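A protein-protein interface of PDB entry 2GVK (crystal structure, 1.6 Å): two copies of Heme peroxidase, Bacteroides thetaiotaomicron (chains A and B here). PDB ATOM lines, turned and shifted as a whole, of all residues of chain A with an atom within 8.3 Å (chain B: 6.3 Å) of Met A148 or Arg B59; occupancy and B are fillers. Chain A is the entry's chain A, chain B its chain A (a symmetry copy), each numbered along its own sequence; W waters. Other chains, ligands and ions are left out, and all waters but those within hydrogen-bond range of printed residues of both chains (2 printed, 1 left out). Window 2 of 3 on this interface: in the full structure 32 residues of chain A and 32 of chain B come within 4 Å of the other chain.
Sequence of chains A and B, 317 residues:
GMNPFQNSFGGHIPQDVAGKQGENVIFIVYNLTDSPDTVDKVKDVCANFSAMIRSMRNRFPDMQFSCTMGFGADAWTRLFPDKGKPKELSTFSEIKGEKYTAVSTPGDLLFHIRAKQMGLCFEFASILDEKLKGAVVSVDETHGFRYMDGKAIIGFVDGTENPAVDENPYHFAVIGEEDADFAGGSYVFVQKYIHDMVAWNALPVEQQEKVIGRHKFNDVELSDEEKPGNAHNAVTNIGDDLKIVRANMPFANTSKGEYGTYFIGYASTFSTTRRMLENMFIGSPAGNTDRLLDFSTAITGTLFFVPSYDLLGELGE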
ATOM      1  N   GLN A  21      -1.809  29.767 -18.476  1.00  0.00           N
ATOM      2  CA  GLN A  21      -2.235  30.113 -17.128  1.00  0.00           C
ATOM      3  C   GLN A  21      -1.683  29.128 -16.106  1.00  0.00           C
ATOM      4  O   GLN A  21      -1.805  27.913 -16.265  1.00  0.00           O
ATOM      5  CB  GLN A  21      -3.762  30.157 -17.044  1.00  0.00           C
ATOM      6  CG  GLN A  21      -4.436  30.727 -18.281  1.00  0.00           C
ATOM      7  CD  GLN A  21      -5.723  30.005 -18.630  1.00  0.00           C
ATOM      8  OE1 GLN A  21      -6.233  29.217 -17.832  1.00  0.00           O
ATOM      9  NE2 GLN A  21      -6.250  30.269 -19.819  1.00  0.00           N
ATOM     10  N   GLU A  23      -0.948  27.192 -12.449  1.00  0.00           N
ATOM     11  CA  GLU A  23      -1.760  26.429 -11.528  1.00  0.00           C
ATOM     12  C   GLU A  23      -2.098  27.303 -10.315  1.00  0.00           C
ATOM     13  O   GLU A  23      -3.172  27.178  -9.723  1.00  0.00           O
ATOM     14  CB  GLU A  23      -1.010  25.175 -11.088  1.00  0.00           C
ATOM     15  CG  GLU A  23      -1.842  24.156 -10.324  1.00  0.00           C
ATOM     16  CD  GLU A  23      -2.876  23.471 -11.192  1.00  0.00           C
ATOM     17  OE1 GLU A  23      -2.614  23.294 -12.396  1.00  0.00           O
ATOM     18  OE2 GLU A  23      -3.957  23.115 -10.672  1.00  0.00           O
ATOM     19  N   PHE A 145      -6.261  30.419  -8.647  1.00  0.00           N
ATOM     20  CA  PHE A 145      -5.939  29.004  -8.787  1.00  0.00           C
ATOM     21  C   PHE A 145      -6.552  28.481 -10.045  1.00  0.00           C
ATOM     22  O   PHE A 145      -7.610  28.951 -10.465  1.00  0.00           O
ATOM     23  CB  PHE A 145      -6.479  28.209  -7.586  1.00  0.00           C
ATOM     24  CG  PHE A 145      -7.942  28.423  -7.326  1.00  0.00           C
ATOM     25  CD1 PHE A 145      -8.372  29.457  -6.525  1.00  0.00           C
ATOM     26  CD2 PHE A 145      -8.896  27.609  -7.930  1.00  0.00           C
ATOM     27  CE1 PHE A 145      -9.728  29.674  -6.327  1.00  0.00           C
ATOM     28  CE2 PHE A 145     -10.216  27.817  -7.729  1.00  0.00           C
ATOM     29  CZ  PHE A 145     -10.644  28.846  -6.929  1.00  0.00           C
ATOM     30  N   ARG A 146      -5.916  27.480 -10.636  1.00  0.00           N
ATOM     31  CA  ARG A 146      -6.512  26.750 -11.748  1.00  0.00           C
ATOM     32  C   ARG A 146      -7.596  25.845 -11.195  1.00  0.00           C
ATOM     33  O   ARG A 146      -7.418  25.179 -10.161  1.00  0.00           O
ATOM     34  CB  ARG A 146      -5.456  25.939 -12.481  1.00  0.00           C
ATOM     35  CG  ARG A 146      -5.926  25.343 -13.780  1.00  0.00           C
ATOM     36  CD  ARG A 146      -4.778  24.604 -14.475  1.00  0.00           C
ATOM     37  NE  ARG A 146      -5.257  23.741 -15.568  1.00  0.00           N
ATOM     38  CZ  ARG A 146      -5.500  24.178 -16.768  1.00  0.00           C
ATOM     39  NH1 ARG A 146      -5.360  25.452 -17.029  1.00  0.00           N
ATOM     40  NH2 ARG A 146      -5.931  23.345 -17.716  1.00  0.00           N
ATOM     41  N   TYR A 147      -8.726  25.823 -11.870  1.00  0.00           N
ATOM     42  CA  TYR A 147      -9.886  25.124 -11.391  1.00  0.00           C
ATOM     43  C   TYR A 147     -10.222  24.003 -12.364  1.00  0.00           C
ATOM     44  O   TYR A 147     -10.663  24.247 -13.487  1.00  0.00           O
ATOM     45  CB  TYR A 147     -11.060  26.121 -11.254  1.00  0.00           C
ATOM     46  CG  TYR A 147     -12.365  25.524 -10.826  1.00  0.00           C
ATOM     47  CD1 TYR A 147     -12.425  24.623  -9.781  1.00  0.00           C
ATOM     48  CD2 TYR A 147     -13.558  25.987 -11.359  1.00  0.00           C
ATOM     49  CE1 TYR A 147     -13.662  24.084  -9.365  1.00  0.00           C
ATOM     50  CE2 TYR A 147     -14.774  25.464 -10.955  1.00  0.00           C
ATOM     51  CZ  TYR A 147     -14.819  24.534  -9.952  1.00  0.00           C
ATOM     52  OH  TYR A 147     -16.026  24.032  -9.557  1.00  0.00           O
ATOM     53  N   MET A 148      -9.941  22.776 -11.947  1.00  0.00           N
ATOM     54  CA  MET A 148     -10.220  21.611 -12.770  1.00  0.00           C
ATOM     55  C   MET A 148      -9.447  21.729 -14.099  1.00  0.00           C
ATOM     56  O   MET A 148      -8.285  22.171 -14.113  1.00  0.00           O
ATOM     57  CB  MET A 148     -11.743  21.484 -13.020  1.00  0.00           C
ATOM     58  CG  MET A 148     -12.594  21.556 -11.750  1.00  0.00           C
ATOM     59  SD  MET A 148     -12.390  19.934 -10.742  1.00  0.00           S
ATOM     60  CE  MET A 148     -12.946  20.539  -8.883  1.00  0.00           C
ATOM     61  N   ASP A 149     -10.119  21.420 -15.199  1.00  0.00           N
ATOM     62  CA  ASP A 149      -9.483  21.418 -16.523  1.00  0.00           C
ATOM     63  C   ASP A 149      -9.550  22.792 -17.166  1.00  0.00           C
ATOM     64  O   ASP A 149     -10.093  22.958 -18.281  1.00  0.00           O
ATOM     65  CB  ASP A 149     -10.124  20.343 -17.445  1.00  0.00           C
ATOM     66  CG  ASP A 149     -11.633  20.544 -17.644  1.00  0.00           C
ATOM     67  OD1 ASP A 149     -12.292  21.063 -16.720  1.00  0.00           O
ATOM     68  OD2 ASP A 149     -12.174  20.119 -18.707  1.00  0.00           O
ATOM     69  N   GLY A 150      -9.062  23.791 -16.447  1.00  0.00           N
ATOM     70  CA  GLY A 150      -9.011  25.159 -16.967  1.00  0.00           C
ATOM     71  C   GLY A 150     -10.346  25.872 -16.965  1.00  0.00           C
ATOM     72  O   GLY A 150     -10.566  26.795 -17.754  1.00  0.00           O
ATOM     73  N   LYS A 151     -11.221  25.502 -16.028  1.00  0.00           N
ATOM     74  CA  LYS A 151     -12.523  26.160 -15.905  1.00  0.00           C
ATOM     75  C   LYS A 151     -12.412  27.509 -15.241  1.00  0.00           C
ATOM     76  O   LYS A 151     -11.620  27.714 -14.318  1.00  0.00           O
ATOM     77  CB  LYS A 151     -13.494  25.289 -15.089  1.00  0.00           C
ATOM     78  CG  LYS A 151     -13.802  23.938 -15.697  1.00  0.00           C
ATOM     79  CD  LYS A 151     -14.856  23.215 -14.875  1.00  0.00           C
ATOM     80  CE  LYS A 151     -14.847  21.682 -15.112  1.00  0.00           C
ATOM     81  NZ  LYS A 151     -15.063  21.323 -16.545  1.00  0.00           N
ATOM     82  N   ALA A 152     -13.222  28.445 -15.718  1.00  0.00           N
ATOM     83  CA  ALA A 152     -13.500  29.636 -14.985  1.00  0.00           C
ATOM     84  C   ALA A 152     -14.394  29.259 -13.789  1.00  0.00           C
ATOM     85  O   ALA A 152     -14.962  28.168 -13.745  1.00  0.00           O
ATOM     86  CB  ALA A 152     -14.187  30.669 -15.869  1.00  0.00           C
ATOM     87  N   GLY A 155     -17.760  27.610 -14.050  1.00  0.00           N
ATOM     88  CA  GLY A 155     -17.862  26.184 -14.388  1.00  0.00           C
ATOM     89  C   GLY A 155     -17.753  25.854 -15.842  1.00  0.00           C
ATOM     90  O   GLY A 155     -18.101  24.758 -16.255  1.00  0.00           O
ATOM     91  N   VAL A 157     -15.071  25.954 -19.165  1.00  0.00           N
ATOM     92  CA  VAL A 157     -13.687  26.080 -19.577  1.00  0.00           C
ATOM     93  C   VAL A 157     -13.473  27.425 -20.210  1.00  0.00           C
ATOM     94  O   VAL A 157     -14.315  27.912 -20.987  1.00  0.00           O
ATOM     95  CB  VAL A 157     -13.305  24.966 -20.582  1.00  0.00           C
ATOM     96  CG1 VAL A 157     -11.951  25.272 -21.267  1.00  0.00           C
ATOM     97  CG2 VAL A 157     -13.291  23.601 -19.874  1.00  0.00           C
ATOM     98  N   PRO A 250      -9.835  32.162 -11.535  1.00  0.00           N
ATOM     99  CA  PRO A 250     -10.704  32.102 -10.383  1.00  0.00           C
ATOM    100  C   PRO A 250     -10.042  32.634  -9.101  1.00  0.00           C
ATOM    101  O   PRO A 250      -8.865  32.413  -8.874  1.00  0.00           O
ATOM    102  CB  PRO A 250     -10.975  30.592 -10.227  1.00  0.00           C
ATOM    103  CG  PRO A 250     -10.716  30.013 -11.521  1.00  0.00           C
ATOM    104  CD  PRO A 250      -9.689  30.845 -12.184  1.00  0.00           C
ATOM    105  N   ARG B  54     -15.549  11.126  -0.184  1.00  0.00           N
ATOM    106  CA  ARG B  54     -15.523   9.998  -1.137  1.00  0.00           C
ATOM    107  C   ARG B  54     -15.554  10.498  -2.563  1.00  0.00           C
ATOM    108  O   ARG B  54     -14.885   9.970  -3.417  1.00  0.00           O
ATOM    109  CB  ARG B  54     -16.706   9.050  -0.912  1.00  0.00           C
ATOM    110  CG  ARG B  54     -16.492   8.013   0.134  1.00  0.00           C
ATOM    111  CD  ARG B  54     -17.553   6.901   0.036  1.00  0.00           C
ATOM    112  NE  ARG B  54     -18.873   7.360   0.481  1.00  0.00           N
ATOM    113  CZ  ARG B  54     -19.231   7.505   1.764  1.00  0.00           C
ATOM    114  NH1 ARG B  54     -18.381   7.211   2.737  1.00  0.00           N
ATOM    115  NH2 ARG B  54     -20.446   7.934   2.072  1.00  0.00           N
ATOM    116  N   SER B  55     -16.411  11.480  -2.820  1.00  0.00           N
ATOM    117  CA  SER B  55     -16.542  12.044  -4.150  1.00  0.00           C
ATOM    118  C   SER B  55     -15.205  12.617  -4.645  1.00  0.00           C
ATOM    119  O   SER B  55     -14.717  12.258  -5.739  1.00  0.00           O
ATOM    120  CB  SER B  55     -17.630  13.119  -4.159  1.00  0.00           C
ATOM    121  OG  SER B  55     -17.733  13.729  -5.435  1.00  0.00           O
ATOM    122  N   MET B  56     -14.563  13.423  -3.810  1.00  0.00           N
ATOM    123  CA  MET B  56     -13.292  14.030  -4.178  1.00  0.00           C
ATOM    124  C   MET B  56     -12.230  12.982  -4.452  1.00  0.00           C
ATOM    125  O   MET B  56     -11.470  13.106  -5.395  1.00  0.00           O
ATOM    126  CB  MET B  56     -12.790  14.951  -3.091  1.00  0.00           C
ATOM    127  CG  MET B  56     -13.675  16.096  -2.790  1.00  0.00           C
ATOM    128  SD  MET B  56     -14.007  17.268  -4.319  1.00  0.00           S
ATOM    129  CE  MET B  56     -12.274  17.614  -4.803  1.00  0.00           C
ATOM    130  N   ARG B  57     -12.149  11.972  -3.586  1.00  0.00           N
ATOM    131  CA  ARG B  57     -11.107  10.942  -3.711  1.00  0.00           C
ATOM    132  C   ARG B  57     -11.377   9.990  -4.871  1.00  0.00           C
ATOM    133  O   ARG B  57     -10.447   9.483  -5.485  1.00  0.00           O
ATOM    134  CB  ARG B  57     -10.959  10.189  -2.415  1.00  0.00           C
ATOM    135  CG  ARG B  57     -10.316  11.020  -1.341  1.00  0.00           C
ATOM    136  CD  ARG B  57     -10.065  10.249  -0.127  1.00  0.00           C
ATOM    137  NE  ARG B  57      -9.553  11.098   0.897  1.00  0.00           N
ATOM    138  CZ  ARG B  57      -9.451  10.767   2.186  1.00  0.00           C
ATOM    139  NH1 ARG B  57      -9.800   9.555   2.597  1.00  0.00           N
ATOM    140  NH2 ARG B  57      -8.978  11.660   3.066  1.00  0.00           N
ATOM    141  N   ASN B  58     -12.645   9.780  -5.192  1.00  0.00           N
ATOM    142  CA  ASN B  58     -13.021   8.979  -6.342  1.00  0.00           C
ATOM    143  C   ASN B  58     -12.661   9.713  -7.642  1.00  0.00           C
ATOM    144  O   ASN B  58     -12.112   9.142  -8.548  1.00  0.00           O
ATOM    145  CB  ASN B  58     -14.525   8.682  -6.291  1.00  0.00           C
ATOM    146  CG  ASN B  58     -15.000   7.910  -7.469  1.00  0.00           C
ATOM    147  OD1 ASN B  58     -14.389   6.937  -7.856  1.00  0.00           O
ATOM    148  ND2 ASN B  58     -16.147   8.330  -8.050  1.00  0.00           N
ATOM    149  N   ARG B  59     -12.925  11.020  -7.671  1.00  0.00           N
ATOM    150  CA  ARG B  59     -12.679  11.826  -8.857  1.00  0.00           C
ATOM    151  C   ARG B  59     -11.190  12.108  -9.067  1.00  0.00           C
ATOM    152  O   ARG B  59     -10.720  12.143 -10.190  1.00  0.00           O
ATOM    153  CB  ARG B  59     -13.439  13.146  -8.757  1.00  0.00           C
ATOM    154  CG  ARG B  59     -14.951  13.005  -8.763  1.00  0.00           C
ATOM    155  CD  ARG B  59     -15.628  14.329  -8.414  1.00  0.00           C
ATOM    156  NE  ARG B  59     -15.362  15.358  -9.427  1.00  0.00           N
ATOM    157  CZ  ARG B  59     -15.625  16.665  -9.281  1.00  0.00           C
ATOM    158  NH1 ARG B  59     -16.126  17.129  -8.152  1.00  0.00           N
ATOM    159  NH2 ARG B  59     -15.354  17.507 -10.269  1.00  0.00           N
ATOM    160  N   PHE B  60     -10.467  12.316  -7.959  1.00  0.00           N
ATOM    161  CA  PHE B  60      -9.048  12.737  -7.986  1.00  0.00           C
ATOM    162  C   PHE B  60      -8.214  11.897  -7.036  1.00  0.00           C
ATOM    163  O   PHE B  60      -7.715  12.387  -6.033  1.00  0.00           O
ATOM    164  CB  PHE B  60      -8.953  14.201  -7.601  1.00  0.00           C
ATOM    165  CG  PHE B  60      -9.951  15.091  -8.342  1.00  0.00           C
ATOM    166  CD1 PHE B  60      -9.738  15.429  -9.642  1.00  0.00           C
ATOM    167  CD2 PHE B  60     -11.106  15.530  -7.717  1.00  0.00           C
ATOM    168  CE1 PHE B  60     -10.695  16.220 -10.352  1.00  0.00           C
ATOM    169  CE2 PHE B  60     -12.032  16.303  -8.402  1.00  0.00           C
ATOM    170  CZ  PHE B  60     -11.817  16.621  -9.729  1.00  0.00           C
ATOM    171  N   PRO B  61      -8.071  10.628  -7.349  1.00  0.00           N
ATOM    172  CA  PRO B  61      -7.436   9.692  -6.432  1.00  0.00           C
ATOM    173  C   PRO B  61      -5.972   9.984  -6.117  1.00  0.00           C
ATOM    174  O   PRO B  61      -5.463   9.485  -5.136  1.00  0.00           O
ATOM    175  CB  PRO B  61      -7.577   8.345  -7.158  1.00  0.00           C
ATOM    176  CG  PRO B  61      -7.867   8.685  -8.566  1.00  0.00           C
ATOM    177  CD  PRO B  61      -8.565   9.973  -8.564  1.00  0.00           C
ATOM    178  N   GLN B 117      -3.951  20.296  -5.145  1.00  0.00           N
ATOM    179  CA  GLN B 117      -4.347  21.458  -5.953  1.00  0.00           C
ATOM    180  C   GLN B 117      -5.356  22.297  -5.206  1.00  0.00           C
ATOM    181  O   GLN B 117      -6.284  21.772  -4.639  1.00  0.00           O
ATOM    182  CB  GLN B 117      -4.943  21.016  -7.264  1.00  0.00           C
ATOM    183  CG  GLN B 117      -3.969  20.356  -8.172  1.00  0.00           C
ATOM    184  CD  GLN B 117      -4.570  20.055  -9.528  1.00  0.00           C
ATOM    185  OE1 GLN B 117      -5.807  20.138  -9.716  1.00  0.00           O
ATOM    186  NE2 GLN B 117      -3.728  19.707 -10.480  1.00  0.00           N
ATOM    187  N   GLY B 119      -7.625  24.178  -6.346  1.00  0.00           N
ATOM    188  CA  GLY B 119      -8.936  24.115  -6.981  1.00  0.00           C
ATOM    189  C   GLY B 119      -9.855  23.066  -6.356  1.00  0.00           C
ATOM    190  O   GLY B 119     -11.082  23.247  -6.289  1.00  0.00           O
ATOM    191  N   LEU B 120      -9.269  21.991  -5.860  1.00  0.00           N
ATOM    192  CA  LEU B 120     -10.056  20.940  -5.200  1.00  0.00           C
ATOM    193  C   LEU B 120     -10.519  21.377  -3.828  1.00  0.00           C
ATOM    194  O   LEU B 120     -11.628  21.054  -3.415  1.00  0.00           O
ATOM    195  CB  LEU B 120      -9.248  19.645  -5.118  1.00  0.00           C
ATOM    196  CG  LEU B 120      -8.754  19.086  -6.459  1.00  0.00           C
ATOM    197  CD1 LEU B 120      -8.107  17.728  -6.227  1.00  0.00           C
ATOM    198  CD2 LEU B 120      -9.858  18.966  -7.477  1.00  0.00           C
ATOM    199  N   GLU B 123     -13.363  23.636  -4.479  1.00  0.00           N
ATOM    200  CA  GLU B 123     -14.558  22.895  -4.863  1.00  0.00           C
ATOM    201  C   GLU B 123     -15.336  22.442  -3.612  1.00  0.00           C
ATOM    202  O   GLU B 123     -16.546  22.690  -3.478  1.00  0.00           O
ATOM    203  CB  GLU B 123     -14.160  21.681  -5.727  1.00  0.00           C
ATOM    204  CG  GLU B 123     -15.294  20.717  -6.045  1.00  0.00           C
ATOM    205  CD  GLU B 123     -16.143  21.183  -7.165  1.00  0.00           C
ATOM    206  OE1 GLU B 123     -16.149  22.410  -7.442  1.00  0.00           O
ATOM    207  OE2 GLU B 123     -16.763  20.316  -7.833  1.00  0.00           O
ATOM    208  N   ILE B 127     -19.105  23.868  -1.921  1.00  0.00           N
ATOM    209  CA  ILE B 127     -20.254  23.034  -1.623  1.00  0.00           C
ATOM    210  C   ILE B 127     -20.680  23.241  -0.154  1.00  0.00           C
ATOM    211  O   ILE B 127     -21.862  23.345   0.133  1.00  0.00           O
ATOM    212  CB  ILE B 127     -19.975  21.567  -1.954  1.00  0.00           C
ATOM    213  CG1 ILE B 127     -19.811  21.411  -3.489  1.00  0.00           C
ATOM    214  CG2 ILE B 127     -21.099  20.687  -1.450  1.00  0.00           C
ATOM    215  CD1 ILE B 127     -19.131  20.152  -3.911  1.00  0.00           C
HETATM  216  O   HOH W   1      -8.296  21.909  -9.481  1.00  0.00           O
HETATM  217  O   HOH W   2      -5.556  24.470  -8.407  1.00  0.00           O
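Water W2 lies within hydrogen-bond range of O of Arg A146, N of Gly B119 and OE2 of Glu A23. Water W1 lies within hydrogen-bond range of OE1 of Gln B117, N of Met A148 and O of Arg A146.
Among the printed residues, merely in contact across the chains: Met A148 with Phe B60 (3.5 Å), Met A148 with Glu B123 (3.6 Å), Phe A145 with Gly B119 (3.6 Å), Arg A146 with Gly B119 (3.7 Å), Met A148 with Leu B120 (3.7 Å), Met A148 with Arg B59 (3.9 Å) and Tyr A147 with Gly B119 (3.99 Å).
No position is printed for both chains.
OE2 of Glu A23 sits close to NE2 of Gln B117 (3.4 Å). The side-chain hydroxyl (OH) of Tyr A147 sits at hydrogen-bond distance from the side-chain carboxylate (OE1) of Glu B123, 2.7 Å away.
Printed residues of chain B within 4 Å of Glu A23: Gln B117. Of the printed residues of chain B, Arg A146 touches Gly B119. Of the printed residues of chain A, Arg B59 touches Met A148. Printed residues of chain A within 4 Å of Phe B60: Met A148 (3.5 Å). Printed residues of chain A within 4 Å of Gly B119: Phe A145 (3.6 Å), Arg A146 (3.7 Å) and Tyr A147 (3.99 Å). Printed residues of chain A within 4 Å of Glu B123: Tyr A147 and Met A148.
Of the 13 printed residues of chain B, 6 touch a printed residue of chain A. Printed residues of chain B that touch a printed residue of chain A: Arg B59, Phe B60, Gln B117, Gly B119, Leu B120 and Glu B123. Hydrophobic or aromatic side chains of chain B within 4 Å of the printed part of chain A: Phe B60 and Leu B120. Of the 13 printed residues of chain A, 5 touch a printed residue of chain B. Printed residues of chain A that touch a printed residue of chain B: Glu A23, Phe A145, Arg A146, Tyr A147 and Met A148. Among the printed residues, no Asp or Glu carboxylate lies within 4 Å of a Lys or Arg side-chain nitrogen of the other chain.
The backbone carbonyl oxygen (O) of Glu A23 sits at hydrogen-bond distance from the backbone NH (N) of Arg A146, 2.9 Å away. The backbone NH (N) of Phe A145 lies within hydrogen-bond range of the backbone carbonyl oxygen (O) of Pro A250, at 3.3 Å. NH1 of Arg B59 is in salt-bridge range of OE2 of Glu B123, at 3.3 Å.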
